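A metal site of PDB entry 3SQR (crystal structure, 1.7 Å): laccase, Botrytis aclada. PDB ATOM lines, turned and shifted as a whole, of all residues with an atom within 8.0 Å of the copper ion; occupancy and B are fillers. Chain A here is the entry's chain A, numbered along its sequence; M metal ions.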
ATOM      1  N   ASP A 273      26.670   8.130 -16.418  1.00  0.00           N
ATOM      2  CA  ASP A 273      26.898   8.482 -17.830  1.00  0.00           C
ATOM      3  C   ASP A 273      28.029   7.690 -18.374  1.00  0.00           C
ATOM      4  O   ASP A 273      29.135   8.186 -18.543  1.00  0.00           O
ATOM      5  CB  ASP A 273      27.187   9.957 -17.970  1.00  0.00           C
ATOM      6  CG  ASP A 273      27.083  10.466 -19.425  1.00  0.00           C
ATOM      7  OD1 ASP A 273      27.009   9.641 -20.346  1.00  0.00           O
ATOM      8  OD2 ASP A 273      27.040  11.690 -19.617  1.00  0.00           O
ATOM      9  N   ILE A 307      23.043   2.524 -20.730  1.00  0.00           N
ATOM     10  CA  ILE A 307      22.652   2.690 -19.350  1.00  0.00           C
ATOM     11  C   ILE A 307      21.247   2.159 -19.115  1.00  0.00           C
ATOM     12  O   ILE A 307      20.319   2.522 -19.811  1.00  0.00           O
ATOM     13  CB  ILE A 307      22.711   4.128 -18.850  1.00  0.00           C
ATOM     14  CG1 ILE A 307      24.126   4.702 -18.995  1.00  0.00           C
ATOM     15  CG2 ILE A 307      22.316   4.140 -17.326  1.00  0.00           C
ATOM     16  CD1 ILE A 307      24.156   6.186 -18.760  1.00  0.00           C
ATOM     17  N   VAL A 394      13.913  15.822 -29.935  1.00  0.00           N
ATOM     18  CA  VAL A 394      14.809  16.268 -28.885  1.00  0.00           C
ATOM     19  C   VAL A 394      15.686  17.410 -29.381  1.00  0.00           C
ATOM     20  O   VAL A 394      16.334  17.318 -30.406  1.00  0.00           O
ATOM     21  CB  VAL A 394      15.676  15.120 -28.376  1.00  0.00           C
ATOM     22  CG1 VAL A 394      16.524  15.555 -27.172  1.00  0.00           C
ATOM     23  CG2 VAL A 394      14.752  13.930 -27.966  1.00  0.00           C
ATOM     24  N   TRP A 404      17.474  19.786 -21.827  1.00  0.00           N
ATOM     25  CA  TRP A 404      16.988  19.102 -23.021  1.00  0.00           C
ATOM     26  C   TRP A 404      15.495  19.376 -23.178  1.00  0.00           C
ATOM     27  O   TRP A 404      14.772  19.455 -22.163  1.00  0.00           O
ATOM     28  CB  TRP A 404      17.210  17.580 -22.916  1.00  0.00           C
ATOM     29  CG  TRP A 404      18.618  17.188 -22.661  1.00  0.00           C
ATOM     30  CD1 TRP A 404      19.176  16.982 -21.453  1.00  0.00           C
ATOM     31  CD2 TRP A 404      19.677  17.078 -23.621  1.00  0.00           C
ATOM     32  NE1 TRP A 404      20.499  16.674 -21.589  1.00  0.00           N
ATOM     33  CE2 TRP A 404      20.841  16.730 -22.906  1.00  0.00           C
ATOM     34  CE3 TRP A 404      19.757  17.252 -25.012  1.00  0.00           C
ATOM     35  CZ2 TRP A 404      22.066  16.552 -23.513  1.00  0.00           C
ATOM     36  CZ3 TRP A 404      20.985  17.052 -25.620  1.00  0.00           C
ATOM     37  CH2 TRP A 404      22.126  16.714 -24.870  1.00  0.00           C
ATOM     38  N   ILE A 461      24.823  12.386 -29.595  1.00  0.00           N
ATOM     39  CA  ILE A 461      24.917  11.488 -28.420  1.00  0.00           C
ATOM     40  C   ILE A 461      23.934  10.315 -28.583  1.00  0.00           C
ATOM     41  O   ILE A 461      22.819  10.529 -29.031  1.00  0.00           O
ATOM     42  CB  ILE A 461      24.624  12.205 -27.120  1.00  0.00           C
ATOM     43  CG1 ILE A 461      25.754  13.241 -26.772  1.00  0.00           C
ATOM     44  CG2 ILE A 461      24.526  11.131 -25.987  1.00  0.00           C
ATOM     45  CD1 ILE A 461      25.323  14.396 -25.855  1.00  0.00           C
ATOM     46  N   TRP A 462      24.340   9.091 -28.232  1.00  0.00           N
ATOM     47  CA  TRP A 462      23.393   7.945 -28.249  1.00  0.00           C
ATOM     48  C   TRP A 462      22.708   7.795 -26.878  1.00  0.00           C
ATOM     49  O   TRP A 462      23.356   7.352 -25.909  1.00  0.00           O
ATOM     50  CB  TRP A 462      24.150   6.649 -28.602  1.00  0.00           C
ATOM     51  CG  TRP A 462      24.564   6.605 -30.018  1.00  0.00           C
ATOM     52  CD1 TRP A 462      25.410   7.453 -30.644  1.00  0.00           C
ATOM     53  CD2 TRP A 462      24.144   5.648 -31.007  1.00  0.00           C
ATOM     54  NE1 TRP A 462      25.595   7.065 -31.959  1.00  0.00           N
ATOM     55  CE2 TRP A 462      24.801   5.978 -32.211  1.00  0.00           C
ATOM     56  CE3 TRP A 462      23.295   4.544 -30.979  1.00  0.00           C
ATOM     57  CZ2 TRP A 462      24.616   5.255 -33.389  1.00  0.00           C
ATOM     58  CZ3 TRP A 462      23.109   3.803 -32.170  1.00  0.00           C
ATOM     59  CH2 TRP A 462      23.769   4.169 -33.348  1.00  0.00           C
ATOM     60  N   HIS A 463      21.450   8.266 -26.779  1.00  0.00           N
ATOM     61  CA  HIS A 463      20.741   8.418 -25.516  1.00  0.00           C
ATOM     62  C   HIS A 463      19.993   7.137 -25.183  1.00  0.00           C
ATOM     63  O   HIS A 463      19.196   6.672 -25.991  1.00  0.00           O
ATOM     64  CB  HIS A 463      19.710   9.567 -25.552  1.00  0.00           C
ATOM     65  CG  HIS A 463      20.287  10.892 -25.921  1.00  0.00           C
ATOM     66  ND1 HIS A 463      20.718  11.793 -24.979  1.00  0.00           N
ATOM     67  CD2 HIS A 463      20.512  11.466 -27.137  1.00  0.00           C
ATOM     68  CE1 HIS A 463      21.226  12.865 -25.593  1.00  0.00           C
ATOM     69  NE2 HIS A 463      21.061  12.708 -26.896  1.00  0.00           N
ATOM     70  N   PRO A 464      20.307   6.514 -24.028  1.00  0.00           N
ATOM     71  CA  PRO A 464      19.597   5.276 -23.630  1.00  0.00           C
ATOM     72  C   PRO A 464      18.186   5.602 -23.167  1.00  0.00           C
ATOM     73  O   PRO A 464      17.975   6.202 -22.093  1.00  0.00           O
ATOM     74  CB  PRO A 464      20.444   4.748 -22.491  1.00  0.00           C
ATOM     75  CG  PRO A 464      21.063   6.027 -21.876  1.00  0.00           C
ATOM     76  CD  PRO A 464      21.352   6.892 -23.052  1.00  0.00           C
ATOM     77  N   ILE A 465      17.208   5.273 -23.991  1.00  0.00           N
ATOM     78  CA  ILE A 465      15.852   5.752 -23.699  1.00  0.00           C
ATOM     79  C   ILE A 465      15.138   4.593 -23.005  1.00  0.00           C
ATOM     80  O   ILE A 465      15.123   3.446 -23.530  1.00  0.00           O
ATOM     81  CB  ILE A 465      15.084   6.075 -25.007  1.00  0.00           C
ATOM     82  CG1 ILE A 465      15.818   7.189 -25.762  1.00  0.00           C
ATOM     83  CG2 ILE A 465      13.596   6.384 -24.720  1.00  0.00           C
ATOM     84  CD1 ILE A 465      15.889   8.492 -24.974  1.00  0.00           C
ATOM     85  N   LEU A 504      18.491   6.027 -28.473  1.00  0.00           N
ATOM     86  CA  LEU A 504      18.212   7.024 -29.519  1.00  0.00           C
ATOM     87  C   LEU A 504      19.562   7.297 -30.194  1.00  0.00           C
ATOM     88  O   LEU A 504      20.449   7.897 -29.591  1.00  0.00           O
ATOM     89  CB  LEU A 504      17.671   8.299 -28.940  1.00  0.00           C
ATOM     90  CG  LEU A 504      17.667   9.545 -29.805  1.00  0.00           C
ATOM     91  CD1 LEU A 504      16.900   9.304 -31.097  1.00  0.00           C
ATOM     92  CD2 LEU A 504      17.085  10.703 -28.970  1.00  0.00           C
ATOM     93  N   HIS A 525      12.358   8.453 -20.725  1.00  0.00           N
ATOM     94  CA  HIS A 525      13.422   9.363 -20.516  1.00  0.00           C
ATOM     95  C   HIS A 525      14.743   8.775 -20.905  1.00  0.00           C
ATOM     96  O   HIS A 525      14.878   7.559 -20.994  1.00  0.00           O
ATOM     97  CB  HIS A 525      13.490   9.773 -19.061  1.00  0.00           C
ATOM     98  CG  HIS A 525      13.823   8.657 -18.137  1.00  0.00           C
ATOM     99  ND1 HIS A 525      15.072   8.483 -17.588  1.00  0.00           N
ATOM    100  CD2 HIS A 525      13.066   7.631 -17.682  1.00  0.00           C
ATOM    101  CE1 HIS A 525      15.048   7.434 -16.786  1.00  0.00           C
ATOM    102  NE2 HIS A 525      13.850   6.876 -16.859  1.00  0.00           N
ATOM    103  N   CYS A 526      15.688   9.674 -21.186  1.00  0.00           N
ATOM    104  CA  CYS A 526      17.090   9.270 -21.279  1.00  0.00           C
ATOM    105  C   CYS A 526      17.564   8.845 -19.882  1.00  0.00           C
ATOM    106  O   CYS A 526      17.269   9.527 -18.877  1.00  0.00           O
ATOM    107  CB  CYS A 526      17.944  10.444 -21.764  1.00  0.00           C
ATOM    108  SG  CYS A 526      19.625   9.937 -21.872  1.00  0.00           S
ATOM    109  N   HIS A 527      18.259   7.726 -19.823  1.00  0.00           N
ATOM    110  CA  HIS A 527      18.723   7.156 -18.575  1.00  0.00           C
ATOM    111  C   HIS A 527      20.111   7.663 -18.192  1.00  0.00           C
ATOM    112  O   HIS A 527      20.663   7.255 -17.130  1.00  0.00           O
ATOM    113  CB  HIS A 527      18.752   5.592 -18.646  1.00  0.00           C
ATOM    114  CG  HIS A 527      18.315   4.917 -17.376  1.00  0.00           C
ATOM    115  ND1 HIS A 527      18.980   5.101 -16.196  1.00  0.00           N
ATOM    116  CD2 HIS A 527      17.297   4.033 -17.112  1.00  0.00           C
ATOM    117  CE1 HIS A 527      18.396   4.382 -15.253  1.00  0.00           C
ATOM    118  NE2 HIS A 527      17.355   3.738 -15.772  1.00  0.00           N
ATOM    119  N   ILE A 528      20.695   8.562 -18.994  1.00  0.00           N
ATOM    120  CA  ILE A 528      21.895   9.257 -18.567  1.00  0.00           C
ATOM    121  C   ILE A 528      21.395  10.226 -17.471  1.00  0.00           C
ATOM    122  O   ILE A 528      20.516  11.063 -17.738  1.00  0.00           O
ATOM    123  CB  ILE A 528      22.566  10.002 -19.712  1.00  0.00           C
ATOM    124  CG1 ILE A 528      23.152   9.045 -20.739  1.00  0.00           C
ATOM    125  CG2 ILE A 528      23.679  10.982 -19.118  1.00  0.00           C
ATOM    126  CD1 ILE A 528      23.611   9.716 -22.080  1.00  0.00           C
ATOM    127  N   ALA A 529      21.847  10.029 -16.247  1.00  0.00           N
ATOM    128  CA  ALA A 529      21.236  10.681 -15.128  1.00  0.00           C
ATOM    129  C   ALA A 529      21.263  12.192 -15.291  1.00  0.00           C
ATOM    130  O   ALA A 529      20.278  12.834 -14.976  1.00  0.00           O
ATOM    131  CB  ALA A 529      21.896  10.240 -13.761  1.00  0.00           C
ATOM    132  N   TRP A 530      22.379  12.731 -15.787  1.00  0.00           N
ATOM    133  CA  TRP A 530      22.419  14.166 -16.052  1.00  0.00           C
ATOM    134  C   TRP A 530      21.320  14.593 -16.998  1.00  0.00           C
ATOM    135  O   TRP A 530      20.713  15.635 -16.728  1.00  0.00           O
ATOM    136  CB  TRP A 530      23.753  14.617 -16.597  1.00  0.00           C
ATOM    137  CG  TRP A 530      24.949  14.101 -15.849  1.00  0.00           C
ATOM    138  CD1 TRP A 530      25.932  13.334 -16.348  1.00  0.00           C
ATOM    139  CD2 TRP A 530      25.304  14.393 -14.493  1.00  0.00           C
ATOM    140  NE1 TRP A 530      26.891  13.125 -15.405  1.00  0.00           N
ATOM    141  CE2 TRP A 530      26.536  13.799 -14.264  1.00  0.00           C
ATOM    142  CE3 TRP A 530      24.742  15.209 -13.499  1.00  0.00           C
ATOM    143  CZ2 TRP A 530      27.198  13.918 -13.050  1.00  0.00           C
ATOM    144  CZ3 TRP A 530      25.383  15.316 -12.306  1.00  0.00           C
ATOM    145  CH2 TRP A 530      26.601  14.659 -12.101  1.00  0.00           C
ATOM    146  N   HIS A 531      21.076  13.808 -18.050  1.00  0.00           N
ATOM    147  CA  HIS A 531      20.101  14.177 -19.091  1.00  0.00           C
ATOM    148  C   HIS A 531      18.697  14.078 -18.549  1.00  0.00           C
ATOM    149  O   HIS A 531      17.882  14.984 -18.758  1.00  0.00           O
ATOM    150  CB  HIS A 531      20.278  13.312 -20.331  1.00  0.00           C
ATOM    151  CG  HIS A 531      21.601  13.528 -21.009  1.00  0.00           C
ATOM    152  ND1 HIS A 531      21.958  12.894 -22.161  1.00  0.00           N
ATOM    153  CD2 HIS A 531      22.671  14.299 -20.654  1.00  0.00           C
ATOM    154  CE1 HIS A 531      23.178  13.275 -22.510  1.00  0.00           C
ATOM    155  NE2 HIS A 531      23.621  14.148 -21.621  1.00  0.00           N
ATOM    156  N   ALA A 532      18.424  13.043 -17.767  1.00  0.00           N
ATOM    157  CA  ALA A 532      17.146  12.955 -17.068  1.00  0.00           C
ATOM    158  C   ALA A 532      16.912  14.149 -16.190  1.00  0.00           C
ATOM    159  O   ALA A 532      15.842  14.765 -16.208  1.00  0.00           O
ATOM    160  CB  ALA A 532      17.069  11.604 -16.227  1.00  0.00           C
ATOM    161  N   GLU A 534      18.211  17.045 -16.460  1.00  0.00           N
ATOM    162  CA  GLU A 534      18.084  18.148 -17.427  1.00  0.00           C
ATOM    163  C   GLU A 534      16.808  18.120 -18.242  1.00  0.00           C
ATOM    164  O   GLU A 534      16.677  18.862 -19.199  1.00  0.00           O
ATOM    165  CB  GLU A 534      19.337  18.159 -18.302  1.00  0.00           C
ATOM    166  CG  GLU A 534      20.530  18.610 -17.501  1.00  0.00           C
ATOM    167  CD  GLU A 534      21.863  18.157 -17.989  1.00  0.00           C
ATOM    168  OE1 GLU A 534      21.957  17.593 -19.089  1.00  0.00           O
ATOM    169  OE2 GLU A 534      22.876  18.371 -17.240  1.00  0.00           O
ATOM    170  N   LEU A 536      15.330  15.552 -20.188  1.00  0.00           N
ATOM    171  CA  LEU A 536      15.134  14.783 -21.377  1.00  0.00           C
ATOM    172  C   LEU A 536      14.182  13.632 -21.118  1.00  0.00           C
ATOM    173  O   LEU A 536      14.604  12.505 -20.905  1.00  0.00           O
ATOM    174  CB  LEU A 536      16.482  14.213 -21.927  1.00  0.00           C
ATOM    175  CG  LEU A 536      16.530  14.044 -23.417  1.00  0.00           C
ATOM    176  CD1 LEU A 536      17.948  13.691 -23.868  1.00  0.00           C
ATOM    177  CD2 LEU A 536      15.581  12.995 -23.903  1.00  0.00           C
HETATM  178 CU    CU M   1      20.711  11.535 -22.989  1.00  0.00          CU
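The backbone NH of Leu 536 sits at hydrogen-bond distance from the backbone carbonyl oxygen of His 531, 3.0 Å away.
The backbone NH (N) of Cys 526 lies within hydrogen-bond range of the backbone carbonyl oxygen (O) of Leu 536 (3.0 Å).
SG of Cys 526 sits close to N of Ile 528 (3.4 Å).
O of His 463 lies within hydrogen-bond range of N of Leu 504 (2.7 Å).
The copper ion is bound by a ring nitrogen (ND1) of His 463, a ring nitrogen (ND1) of His 531 and the side-chain sulfur (SG) of Cys 526.
Merely in contact with the copper ion: Ile 528 (3.5 Å) and Leu 536 (3.6 Å).
Of the 20 residues printed, 5 come within 4 Å of the copper ion.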
